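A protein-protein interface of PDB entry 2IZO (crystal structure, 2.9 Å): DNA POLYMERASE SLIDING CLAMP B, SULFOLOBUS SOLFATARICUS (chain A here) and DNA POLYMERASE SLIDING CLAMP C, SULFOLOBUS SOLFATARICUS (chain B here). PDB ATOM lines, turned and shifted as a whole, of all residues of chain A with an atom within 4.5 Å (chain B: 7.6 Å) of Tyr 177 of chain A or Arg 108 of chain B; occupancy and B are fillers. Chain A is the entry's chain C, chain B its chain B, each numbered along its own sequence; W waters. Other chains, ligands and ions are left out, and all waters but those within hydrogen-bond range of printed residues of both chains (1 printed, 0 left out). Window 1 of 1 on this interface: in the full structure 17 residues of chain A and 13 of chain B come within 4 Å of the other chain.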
ATOM      1  N   VAL A 145       0.714   1.759 -17.694  1.00  0.00           N
ATOM      2  CA  VAL A 145       1.703   1.051 -16.888  1.00  0.00           C
ATOM      3  C   VAL A 145       1.004   0.221 -15.812  1.00  0.00           C
ATOM      4  O   VAL A 145       1.144  -0.999 -15.783  1.00  0.00           O
ATOM      5  CB  VAL A 145       2.759   2.019 -16.272  1.00  0.00           C
ATOM      6  CG1 VAL A 145       3.642   1.310 -15.254  1.00  0.00           C
ATOM      7  CG2 VAL A 145       3.626   2.633 -17.361  1.00  0.00           C
ATOM      8  N   ILE A 146       0.232   0.880 -14.954  1.00  0.00           N
ATOM      9  CA  ILE A 146      -0.504   0.196 -13.890  1.00  0.00           C
ATOM     10  C   ILE A 146      -1.363  -0.952 -14.437  1.00  0.00           C
ATOM     11  O   ILE A 146      -1.359  -2.049 -13.876  1.00  0.00           O
ATOM     12  CB  ILE A 146      -1.387   1.173 -13.075  1.00  0.00           C
ATOM     13  CG1 ILE A 146      -0.519   2.246 -12.414  1.00  0.00           C
ATOM     14  CG2 ILE A 146      -2.192   0.422 -12.016  1.00  0.00           C
ATOM     15  CD1 ILE A 146      -1.295   3.421 -11.849  1.00  0.00           C
ATOM     16  N   ASP A 149       0.769  -3.817 -15.309  1.00  0.00           N
ATOM     17  CA  ASP A 149       1.350  -4.351 -14.085  1.00  0.00           C
ATOM     18  C   ASP A 149       0.382  -5.255 -13.335  1.00  0.00           C
ATOM     19  O   ASP A 149       0.769  -6.335 -12.875  1.00  0.00           O
ATOM     20  CB  ASP A 149       1.802  -3.223 -13.158  1.00  0.00           C
ATOM     21  CG  ASP A 149       3.033  -2.494 -13.662  1.00  0.00           C
ATOM     22  OD1 ASP A 149       3.300  -1.389 -13.148  1.00  0.00           O
ATOM     23  OD2 ASP A 149       3.729  -3.012 -14.558  1.00  0.00           O
ATOM     24  N   VAL A 150      -0.873  -4.814 -13.219  1.00  0.00           N
ATOM     25  CA  VAL A 150      -1.879  -5.549 -12.440  1.00  0.00           C
ATOM     26  C   VAL A 150      -2.306  -6.865 -13.095  1.00  0.00           C
ATOM     27  O   VAL A 150      -2.370  -7.899 -12.425  1.00  0.00           O
ATOM     28  CB  VAL A 150      -3.113  -4.678 -12.046  1.00  0.00           C
ATOM     29  CG1 VAL A 150      -2.700  -3.564 -11.085  1.00  0.00           C
ATOM     30  CG2 VAL A 150      -3.821  -4.107 -13.268  1.00  0.00           C
ATOM     31  N   VAL A 153       0.079  -9.734 -12.616  1.00  0.00           N
ATOM     32  CA  VAL A 153       0.202 -10.320 -11.286  1.00  0.00           C
ATOM     33  C   VAL A 153      -1.045 -11.115 -10.864  1.00  0.00           C
ATOM     34  O   VAL A 153      -0.926 -12.201 -10.281  1.00  0.00           O
ATOM     35  CB  VAL A 153       0.592  -9.232 -10.250  1.00  0.00           C
ATOM     36  CG1 VAL A 153       0.471  -9.742  -8.831  1.00  0.00           C
ATOM     37  CG2 VAL A 153       2.014  -8.754 -10.508  1.00  0.00           C
ATOM     38  N   ILE A 168      -2.717   1.382  -5.085  1.00  0.00           N
ATOM     39  CA  ILE A 168      -3.216   0.378  -6.014  1.00  0.00           C
ATOM     40  C   ILE A 168      -2.540  -0.942  -5.692  1.00  0.00           C
ATOM     41  O   ILE A 168      -1.325  -0.995  -5.538  1.00  0.00           O
ATOM     42  CB  ILE A 168      -3.016   0.814  -7.489  1.00  0.00           C
ATOM     43  CG1 ILE A 168      -4.073   1.864  -7.858  1.00  0.00           C
ATOM     44  CG2 ILE A 168      -3.109  -0.380  -8.434  1.00  0.00           C
ATOM     45  CD1 ILE A 168      -3.802   2.642  -9.133  1.00  0.00           C
ATOM     46  N   GLU A 169      -3.345  -1.994  -5.561  1.00  0.00           N
ATOM     47  CA  GLU A 169      -2.860  -3.312  -5.168  1.00  0.00           C
ATOM     48  C   GLU A 169      -3.440  -4.419  -6.026  1.00  0.00           C
ATOM     49  O   GLU A 169      -4.598  -4.359  -6.451  1.00  0.00           O
ATOM     50  CB  GLU A 169      -3.204  -3.600  -3.712  1.00  0.00           C
ATOM     51  CG  GLU A 169      -2.385  -2.829  -2.699  1.00  0.00           C
ATOM     52  CD  GLU A 169      -2.761  -3.181  -1.273  1.00  0.00           C
ATOM     53  OE1 GLU A 169      -3.977  -3.229  -0.978  1.00  0.00           O
ATOM     54  OE2 GLU A 169      -1.843  -3.411  -0.449  1.00  0.00           O
ATOM     55  N   ALA A 170      -2.611  -5.429  -6.267  1.00  0.00           N
ATOM     56  CA  ALA A 170      -3.007  -6.646  -6.951  1.00  0.00           C
ATOM     57  C   ALA A 170      -2.194  -7.763  -6.314  1.00  0.00           C
ATOM     58  O   ALA A 170      -1.273  -7.489  -5.543  1.00  0.00           O
ATOM     59  CB  ALA A 170      -2.715  -6.539  -8.435  1.00  0.00           C
ATOM     60  N   ARG A 176       2.548 -10.201  -4.803  1.00  0.00           N
ATOM     61  CA  ARG A 176       1.708  -9.002  -4.851  1.00  0.00           C
ATOM     62  C   ARG A 176       2.268  -7.888  -5.738  1.00  0.00           C
ATOM     63  O   ARG A 176       3.407  -7.955  -6.212  1.00  0.00           O
ATOM     64  CB  ARG A 176       1.475  -8.451  -3.431  1.00  0.00           C
ATOM     65  CG  ARG A 176       0.970  -9.456  -2.377  1.00  0.00           C
ATOM     66  CD  ARG A 176      -0.501  -9.858  -2.555  1.00  0.00           C
ATOM     67  NE  ARG A 176      -1.376  -8.718  -2.848  1.00  0.00           N
ATOM     68  CZ  ARG A 176      -2.708  -8.756  -2.839  1.00  0.00           C
ATOM     69  NH1 ARG A 176      -3.352  -9.878  -2.535  1.00  0.00           N
ATOM     70  NH2 ARG A 176      -3.401  -7.661  -3.126  1.00  0.00           N
ATOM     71  N   TYR A 177       1.439  -6.870  -5.953  1.00  0.00           N
ATOM     72  CA  TYR A 177       1.833  -5.628  -6.605  1.00  0.00           C
ATOM     73  C   TYR A 177       1.283  -4.451  -5.808  1.00  0.00           C
ATOM     74  O   TYR A 177       0.124  -4.466  -5.389  1.00  0.00           O
ATOM     75  CB  TYR A 177       1.297  -5.574  -8.034  1.00  0.00           C
ATOM     76  CG  TYR A 177       1.485  -4.229  -8.705  1.00  0.00           C
ATOM     77  CD1 TYR A 177       2.738  -3.826  -9.163  1.00  0.00           C
ATOM     78  CD2 TYR A 177       0.411  -3.356  -8.879  1.00  0.00           C
ATOM     79  CE1 TYR A 177       2.916  -2.592  -9.780  1.00  0.00           C
ATOM     80  CE2 TYR A 177       0.581  -2.119  -9.496  1.00  0.00           C
ATOM     81  CZ  TYR A 177       1.836  -1.750  -9.944  1.00  0.00           C
ATOM     82  OH  TYR A 177       2.014  -0.536 -10.557  1.00  0.00           O
ATOM     83  N   VAL A 178       2.120  -3.439  -5.597  1.00  0.00           N
ATOM     84  CA  VAL A 178       1.704  -2.222  -4.898  1.00  0.00           C
ATOM     85  C   VAL A 178       2.182  -0.975  -5.643  1.00  0.00           C
ATOM     86  O   VAL A 178       3.346  -0.884  -6.037  1.00  0.00           O
ATOM     87  CB  VAL A 178       2.225  -2.171  -3.436  1.00  0.00           C
ATOM     88  CG1 VAL A 178       1.414  -1.167  -2.622  1.00  0.00           C
ATOM     89  CG2 VAL A 178       2.179  -3.551  -2.774  1.00  0.00           C
ATOM     90  N   ALA A 179       1.278  -0.022  -5.836  1.00  0.00           N
ATOM     91  CA  ALA A 179       1.617   1.249  -6.469  1.00  0.00           C
ATOM     92  C   ALA A 179       1.070   2.417  -5.662  1.00  0.00           C
ATOM     93  O   ALA A 179      -0.068   2.381  -5.182  1.00  0.00           O
ATOM     94  CB  ALA A 179       1.094   1.296  -7.893  1.00  0.00           C
ATOM     95  N   ILE B  79       8.579  -9.503 -14.154  1.00  0.00           N
ATOM     96  CA  ILE B  79       8.548  -8.290 -13.351  1.00  0.00           C
ATOM     97  C   ILE B  79       9.535  -7.291 -13.942  1.00  0.00           C
ATOM     98  O   ILE B  79       9.167  -6.154 -14.248  1.00  0.00           O
ATOM     99  CB  ILE B  79       8.820  -8.583 -11.852  1.00  0.00           C
ATOM    100  CG1 ILE B  79       7.580  -9.229 -11.224  1.00  0.00           C
ATOM    101  CG2 ILE B  79       9.187  -7.305 -11.095  1.00  0.00           C
ATOM    102  CD1 ILE B  79       7.864 -10.171 -10.089  1.00  0.00           C
ATOM    103  N   LYS B  81      10.596  -7.151 -16.836  1.00  0.00           N
ATOM    104  CA  LYS B  81      10.122  -6.716 -18.156  1.00  0.00           C
ATOM    105  C   LYS B  81       9.220  -5.470 -18.098  1.00  0.00           C
ATOM    106  O   LYS B  81       8.903  -4.881 -19.133  1.00  0.00           O
ATOM    107  CB  LYS B  81       9.415  -7.864 -18.882  1.00  0.00           C
ATOM    108  N   ARG B  82       8.823  -5.067 -16.890  1.00  0.00           N
ATOM    109  CA  ARG B  82       7.906  -3.936 -16.710  1.00  0.00           C
ATOM    110  C   ARG B  82       8.648  -2.640 -16.379  1.00  0.00           C
ATOM    111  O   ARG B  82       8.027  -1.612 -16.094  1.00  0.00           O
ATOM    112  CB  ARG B  82       6.853  -4.247 -15.636  1.00  0.00           C
ATOM    113  CG  ARG B  82       5.970  -5.456 -15.930  1.00  0.00           C
ATOM    114  CD  ARG B  82       4.641  -5.097 -16.591  1.00  0.00           C
ATOM    115  NE  ARG B  82       4.796  -4.451 -17.893  1.00  0.00           N
ATOM    116  CZ  ARG B  82       4.443  -3.197 -18.162  1.00  0.00           C
ATOM    117  NH1 ARG B  82       3.902  -2.426 -17.224  1.00  0.00           N
ATOM    118  NH2 ARG B  82       4.629  -2.712 -19.381  1.00  0.00           N
ATOM    119  N   VAL B  83       9.976  -2.704 -16.431  1.00  0.00           N
ATOM    120  CA  VAL B  83      10.834  -1.538 -16.209  1.00  0.00           C
ATOM    121  C   VAL B  83      10.591  -0.445 -17.253  1.00  0.00           C
ATOM    122  O   VAL B  83      10.374  -0.738 -18.433  1.00  0.00           O
ATOM    123  CB  VAL B  83      12.344  -1.931 -16.173  1.00  0.00           C
ATOM    124  CG1 VAL B  83      12.827  -2.456 -17.540  1.00  0.00           C
ATOM    125  CG2 VAL B  83      13.196  -0.761 -15.700  1.00  0.00           C
ATOM    126  N   LEU B  84      10.612   0.806 -16.803  1.00  0.00           N
ATOM    127  CA  LEU B  84      10.499   1.958 -17.692  1.00  0.00           C
ATOM    128  C   LEU B  84      11.877   2.558 -17.976  1.00  0.00           C
ATOM    129  O   LEU B  84      12.865   2.193 -17.329  1.00  0.00           O
ATOM    130  CB  LEU B  84       9.555   3.012 -17.106  1.00  0.00           C
ATOM    131  CG  LEU B  84       8.047   2.746 -17.154  1.00  0.00           C
ATOM    132  CD1 LEU B  84       7.284   3.845 -16.424  1.00  0.00           C
ATOM    133  CD2 LEU B  84       7.534   2.605 -18.582  1.00  0.00           C
ATOM    134  N   LYS B  85      11.927   3.473 -18.945  1.00  0.00           N
ATOM    135  CA  LYS B  85      13.180   4.077 -19.404  1.00  0.00           C
ATOM    136  C   LYS B  85      13.941   4.802 -18.294  1.00  0.00           C
ATOM    137  O   LYS B  85      15.141   4.575 -18.111  1.00  0.00           O
ATOM    138  CB  LYS B  85      12.918   5.022 -20.575  1.00  0.00           C
ATOM    139  N   ASP B  87      13.374   4.631 -15.010  1.00  0.00           N
ATOM    140  CA  ASP B  87      13.256   3.947 -13.725  1.00  0.00           C
ATOM    141  C   ASP B  87      14.577   3.433 -13.151  1.00  0.00           C
ATOM    142  O   ASP B  87      15.553   3.225 -13.879  1.00  0.00           O
ATOM    143  CB  ASP B  87      12.257   2.798 -13.833  1.00  0.00           C
ATOM    144  CG  ASP B  87      10.813   3.264 -13.750  1.00  0.00           C
ATOM    145  OD1 ASP B  87       9.929   2.390 -13.632  1.00  0.00           O
ATOM    146  OD2 ASP B  87      10.552   4.490 -13.804  1.00  0.00           O
ATOM    147  N   THR B  88      14.593   3.250 -11.832  1.00  0.00           N
ATOM    148  CA  THR B  88      15.728   2.660 -11.126  1.00  0.00           C
ATOM    149  C   THR B  88      15.242   1.512 -10.242  1.00  0.00           C
ATOM    150  O   THR B  88      14.391   1.707  -9.372  1.00  0.00           O
ATOM    151  CB  THR B  88      16.485   3.702 -10.267  1.00  0.00           C
ATOM    152  OG1 THR B  88      15.575   4.345  -9.371  1.00  0.00           O
ATOM    153  CG2 THR B  88      17.139   4.754 -11.147  1.00  0.00           C
ATOM    154  N   LEU B  89      15.777   0.319 -10.477  1.00  0.00           N
ATOM    155  CA  LEU B  89      15.363  -0.872  -9.740  1.00  0.00           C
ATOM    156  C   LEU B  89      15.993  -0.974  -8.352  1.00  0.00           C
ATOM    157  O   LEU B  89      17.186  -0.728  -8.176  1.00  0.00           O
ATOM    158  CB  LEU B  89      15.684  -2.132 -10.550  1.00  0.00           C
ATOM    159  CG  LEU B  89      15.420  -3.493  -9.909  1.00  0.00           C
ATOM    160  CD1 LEU B  89      13.929  -3.734  -9.758  1.00  0.00           C
ATOM    161  CD2 LEU B  89      16.061  -4.580 -10.738  1.00  0.00           C
ATOM    162  N   ILE B  90      15.189  -1.345  -7.364  1.00  0.00           N
ATOM    163  CA  ILE B  90      15.735  -1.605  -6.035  1.00  0.00           C
ATOM    164  C   ILE B  90      15.286  -2.950  -5.477  1.00  0.00           C
ATOM    165  O   ILE B  90      14.095  -3.186  -5.259  1.00  0.00           O
ATOM    166  CB  ILE B  90      15.542  -0.408  -5.028  1.00  0.00           C
ATOM    167  CG1 ILE B  90      15.620  -0.892  -3.574  1.00  0.00           C
ATOM    168  CG2 ILE B  90      14.246   0.364  -5.295  1.00  0.00           C
ATOM    169  CD1 ILE B  90      15.959   0.199  -2.578  1.00  0.00           C
ATOM    170  N   THR B  99      11.436  -8.605  -3.029  1.00  0.00           N
ATOM    171  CA  THR B  99      10.750  -7.426  -3.545  1.00  0.00           C
ATOM    172  C   THR B  99      11.592  -6.693  -4.588  1.00  0.00           C
ATOM    173  O   THR B  99      12.778  -6.412  -4.368  1.00  0.00           O
ATOM    174  CB  THR B  99      10.372  -6.446  -2.402  1.00  0.00           C
ATOM    175  OG1 THR B  99       9.642  -7.142  -1.378  1.00  0.00           O
ATOM    176  CG2 THR B  99       9.526  -5.299  -2.934  1.00  0.00           C
ATOM    177  N   LEU B 100      10.970  -6.395  -5.726  1.00  0.00           N
ATOM    178  CA  LEU B 100      11.591  -5.565  -6.748  1.00  0.00           C
ATOM    179  C   LEU B 100      10.753  -4.307  -6.945  1.00  0.00           C
ATOM    180  O   LEU B 100       9.561  -4.382  -7.255  1.00  0.00           O
ATOM    181  CB  LEU B 100      11.754  -6.328  -8.067  1.00  0.00           C
ATOM    182  CG  LEU B 100      12.393  -7.726  -8.064  1.00  0.00           C
ATOM    183  CD1 LEU B 100      12.447  -8.282  -9.477  1.00  0.00           C
ATOM    184  CD2 LEU B 100      13.781  -7.745  -7.445  1.00  0.00           C
ATOM    185  N   THR B 101      11.388  -3.157  -6.748  1.00  0.00           N
ATOM    186  CA  THR B 101      10.719  -1.865  -6.788  1.00  0.00           C
ATOM    187  C   THR B 101      11.281  -0.982  -7.895  1.00  0.00           C
ATOM    188  O   THR B 101      12.484  -0.717  -7.929  1.00  0.00           O
ATOM    189  CB  THR B 101      10.908  -1.120  -5.455  1.00  0.00           C
ATOM    190  OG1 THR B 101      10.554  -1.982  -4.370  1.00  0.00           O
ATOM    191  CG2 THR B 101      10.059   0.139  -5.406  1.00  0.00           C
ATOM    192  N   PHE B 102      10.405  -0.524  -8.790  1.00  0.00           N
ATOM    193  CA  PHE B 102      10.771   0.484  -9.779  1.00  0.00           C
ATOM    194  C   PHE B 102      10.462   1.892  -9.257  1.00  0.00           C
ATOM    195  O   PHE B 102       9.340   2.177  -8.832  1.00  0.00           O
ATOM    196  CB  PHE B 102      10.042   0.233 -11.101  1.00  0.00           C
ATOM    197  CG  PHE B 102      10.309  -1.121 -11.695  1.00  0.00           C
ATOM    198  CD1 PHE B 102       9.281  -2.052 -11.819  1.00  0.00           C
ATOM    199  CD2 PHE B 102      11.587  -1.470 -12.135  1.00  0.00           C
ATOM    200  CE1 PHE B 102       9.521  -3.310 -12.367  1.00  0.00           C
ATOM    201  CE2 PHE B 102      11.837  -2.729 -12.684  1.00  0.00           C
ATOM    202  CZ  PHE B 102      10.801  -3.647 -12.798  1.00  0.00           C
ATOM    203  N   ASP B 103      11.465   2.765  -9.281  1.00  0.00           N
ATOM    204  CA  ASP B 103      11.284   4.148  -8.846  1.00  0.00           C
ATOM    205  C   ASP B 103      11.577   5.150  -9.968  1.00  0.00           C
ATOM    206  O   ASP B 103      12.723   5.287 -10.412  1.00  0.00           O
ATOM    207  CB  ASP B 103      12.148   4.451  -7.618  1.00  0.00           C
ATOM    208  CG  ASP B 103      11.859   5.823  -7.026  1.00  0.00           C
ATOM    209  OD1 ASP B 103      12.776   6.673  -7.022  1.00  0.00           O
ATOM    210  OD2 ASP B 103      10.712   6.056  -6.581  1.00  0.00           O
ATOM    211  N   GLY B 104      10.534   5.847 -10.412  1.00  0.00           N
ATOM    212  CA  GLY B 104      10.652   6.869 -11.449  1.00  0.00           C
ATOM    213  C   GLY B 104       9.646   7.986 -11.245  1.00  0.00           C
ATOM    214  O   GLY B 104       9.669   8.665 -10.217  1.00  0.00           O
ATOM    215  N   GLU B 105       8.758   8.172 -12.223  1.00  0.00           N
ATOM    216  CA  GLU B 105       7.689   9.170 -12.130  1.00  0.00           C
ATOM    217  C   GLU B 105       6.824   8.874 -10.905  1.00  0.00           C
ATOM    218  O   GLU B 105       6.352   9.787 -10.227  1.00  0.00           O
ATOM    219  CB  GLU B 105       6.843   9.187 -13.411  1.00  0.00           C
ATOM    220  CG  GLU B 105       5.951  10.425 -13.556  1.00  0.00           C
ATOM    221  CD  GLU B 105       5.099  10.428 -14.828  1.00  0.00           C
ATOM    222  OE1 GLU B 105       5.194   9.472 -15.634  1.00  0.00           O
ATOM    223  OE2 GLU B 105       4.331  11.399 -15.018  1.00  0.00           O
ATOM    224  N   PHE B 106       6.633   7.584 -10.642  1.00  0.00           N
ATOM    225  CA  PHE B 106       6.023   7.104  -9.409  1.00  0.00           C
ATOM    226  C   PHE B 106       6.651   5.773  -9.011  1.00  0.00           C
ATOM    227  O   PHE B 106       7.398   5.178  -9.787  1.00  0.00           O
ATOM    228  CB  PHE B 106       4.492   7.006  -9.527  1.00  0.00           C
ATOM    229  CG  PHE B 106       4.005   6.040 -10.582  1.00  0.00           C
ATOM    230  CD1 PHE B 106       3.949   6.418 -11.925  1.00  0.00           C
ATOM    231  CD2 PHE B 106       3.569   4.769 -10.226  1.00  0.00           C
ATOM    232  CE1 PHE B 106       3.490   5.534 -12.900  1.00  0.00           C
ATOM    233  CE2 PHE B 106       3.109   3.874 -11.198  1.00  0.00           C
ATOM    234  CZ  PHE B 106       3.069   4.260 -12.536  1.00  0.00           C
ATOM    235  N   THR B 107       6.353   5.324  -7.795  1.00  0.00           N
ATOM    236  CA  THR B 107       6.923   4.100  -7.237  1.00  0.00           C
ATOM    237  C   THR B 107       5.961   2.927  -7.406  1.00  0.00           C
ATOM    238  O   THR B 107       4.761   3.055  -7.155  1.00  0.00           O
ATOM    239  CB  THR B 107       7.246   4.281  -5.737  1.00  0.00           C
ATOM    240  OG1 THR B 107       7.990   5.490  -5.548  1.00  0.00           O
ATOM    241  CG2 THR B 107       8.058   3.114  -5.206  1.00  0.00           C
ATOM    242  N   ARG B 108       6.495   1.791  -7.844  1.00  0.00           N
ATOM    243  CA  ARG B 108       5.720   0.552  -7.950  1.00  0.00           C
ATOM    244  C   ARG B 108       6.602  -0.659  -7.690  1.00  0.00           C
ATOM    245  O   ARG B 108       7.605  -0.859  -8.372  1.00  0.00           O
ATOM    246  CB  ARG B 108       5.030   0.436  -9.317  1.00  0.00           C
ATOM    247  CG  ARG B 108       5.748   1.168 -10.435  1.00  0.00           C
ATOM    248  CD  ARG B 108       5.449   0.590 -11.790  1.00  0.00           C
ATOM    249  NE  ARG B 108       6.486   0.973 -12.741  1.00  0.00           N
ATOM    250  CZ  ARG B 108       6.785   0.299 -13.845  1.00  0.00           C
ATOM    251  NH1 ARG B 108       7.751   0.735 -14.638  1.00  0.00           N
ATOM    252  NH2 ARG B 108       6.128  -0.810 -14.161  1.00  0.00           N
ATOM    253  N   SER B 109       6.220  -1.461  -6.698  1.00  0.00           N
ATOM    254  CA  SER B 109       6.979  -2.660  -6.332  1.00  0.00           C
ATOM    255  C   SER B 109       6.201  -3.969  -6.477  1.00  0.00           C
ATOM    256  O   SER B 109       4.986  -4.011  -6.287  1.00  0.00           O
ATOM    257  CB  SER B 109       7.539  -2.539  -4.917  1.00  0.00           C
ATOM    258  OG  SER B 109       6.573  -2.030  -4.023  1.00  0.00           O
ATOM    259  N   PHE B 110       6.930  -5.027  -6.829  1.00  0.00           N
ATOM    260  CA  PHE B 110       6.381  -6.375  -6.972  1.00  0.00           C
ATOM    261  C   PHE B 110       7.006  -7.278  -5.915  1.00  0.00           C
ATOM    262  O   PHE B 110       8.221  -7.245  -5.710  1.00  0.00           O
ATOM    263  CB  PHE B 110       6.713  -6.948  -8.355  1.00  0.00           C
ATOM    264  CG  PHE B 110       6.124  -6.179  -9.508  1.00  0.00           C
ATOM    265  CD1 PHE B 110       6.663  -4.956  -9.903  1.00  0.00           C
ATOM    266  CD2 PHE B 110       5.050  -6.695 -10.220  1.00  0.00           C
ATOM    267  CE1 PHE B 110       6.126  -4.250 -10.974  1.00  0.00           C
ATOM    268  CE2 PHE B 110       4.506  -5.998 -11.297  1.00  0.00           C
ATOM    269  CZ  PHE B 110       5.049  -4.772 -11.676  1.00  0.00           C
ATOM    270  N   GLU B 111       6.183  -8.095  -5.262  1.00  0.00           N
ATOM    271  CA  GLU B 111       6.676  -9.046  -4.265  1.00  0.00           C
ATOM    272  C   GLU B 111       6.526 -10.478  -4.737  1.00  0.00           C
ATOM    273  O   GLU B 111       5.499 -10.844  -5.299  1.00  0.00           O
ATOM    274  CB  GLU B 111       5.948  -8.872  -2.934  1.00  0.00           C
ATOM    275  CG  GLU B 111       5.951  -7.443  -2.418  1.00  0.00           C
ATOM    276  CD  GLU B 111       5.890  -7.355  -0.907  1.00  0.00           C
ATOM    277  OE1 GLU B 111       5.096  -8.098  -0.286  1.00  0.00           O
ATOM    278  OE2 GLU B 111       6.643  -6.527  -0.347  1.00  0.00           O
HETATM  279  O   HOH W   1       4.683 -10.190  -8.022  1.00  0.00           O
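The guanidinium group (NH1) of Arg 82 of chain B is in hydrogen-bond range of the backbone carbonyl oxygen (O) of Val 145 of chain A (3.4 Å).
The guanidinium group of Arg 82 of chain B is in salt-bridge range of the side-chain carboxylate of Asp 149 of chain A, 2.7 Å away.
NH2 of Arg 108 of chain B lies within salt-bridge range of OD1 of Asp 149 of chain A, 3.1 Å away.
N of Val 178 of chain A is in hydrogen-bond range of O of Ser 109 of chain B, 3.0 Å away.
The backbone carbonyl oxygen of Arg 176 of chain A sits at hydrogen-bond distance from the backbone NH of Glu 111 of chain B, 2.9 Å away.
The backbone carbonyl oxygen of Arg 82 of chain B sits at hydrogen-bond distance from the guanidinium group of Arg 108 of chain B, 2.8 Å away.
The side-chain carboxylate (OD1) of Asp 87 of chain B is in salt-bridge range of the guanidinium group (NH1) of Arg 108 of chain B, 2.9 Å away.
The backbone carbonyl oxygen (O) of Leu 100 of chain B is in hydrogen-bond range of the backbone NH (N) of Phe 110 of chain B (2.7 Å).
The backbone NH (N) of Phe 102 of chain B lies within hydrogen-bond range of the backbone carbonyl oxygen (O) of Arg 108 of chain B (2.9 Å).
The side-chain carboxylate of Asp 149 of chain A sits at hydrogen-bond distance from the side-chain hydroxyl of Tyr 177 of chain A (3.0 Å).
The backbone carbonyl oxygen of Ala 170 of chain A sits at hydrogen-bond distance from the backbone NH of Tyr 177 of chain A, 2.8 Å away.
Among the printed residues, merely in contact across the chains: Val 145 of chain A with Leu 84 of chain B, Val 145 of chain A with Arg 108 of chain B, Asp 149 of chain A with Phe 110 of chain B, Val 153 of chain A with Phe 110 of chain B, Arg 176 of chain A with Phe 110 of chain B, Tyr 177 of chain A with Arg 108 of chain B, Tyr 177 of chain A with Ser 109 of chain B, Tyr 177 of chain A with Phe 110 of chain B, Val 178 of chain A with Arg 108 of chain B and Ala 179 of chain A with Thr 107 of chain B.
Tyr 177 of chain A touches three residues of chain B.
Of the printed residues of chain A, Arg 82 of chain B touches Val 145 and Asp 149.
Of the printed residues of chain B, Asp 149 of chain A touches Arg 82 (2.7 Å), Arg 108 (3.1 Å) and Phe 110 (3.6 Å).
Leu 89 of chain B touches none of the printed residues of chain A.
Phe 102 of chain B touches none of the printed residues of chain A.
The nearest residue of chain B that does not touch Tyr 177 of chain A is Phe 106 of chain B (4.6 Å).
The nearest residue of chain A that does not touch Arg 108 of chain B is Ala 179 of chain A (4.3 Å).
The nearest printed residue of chain A that does not touch Leu 84 of chain B is Asp 149 of chain A (7.3 Å).
Hydrophobic or aromatic side chains of chain A that line the printed part of chain B: Val 145, Val 153 and Tyr 177.
Hydrophobic or aromatic side chains of chain B within 4 Å of the printed part of chain A: Leu 84 and Phe 110.
Along chain B the printed residues that touch a printed residue of chain A span positions 82 to 111.
Water W1 lies within hydrogen-bond range of O of Glu 111 of chain B (2.9 Å) and O of Arg 176 of chain A (3.1 Å).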
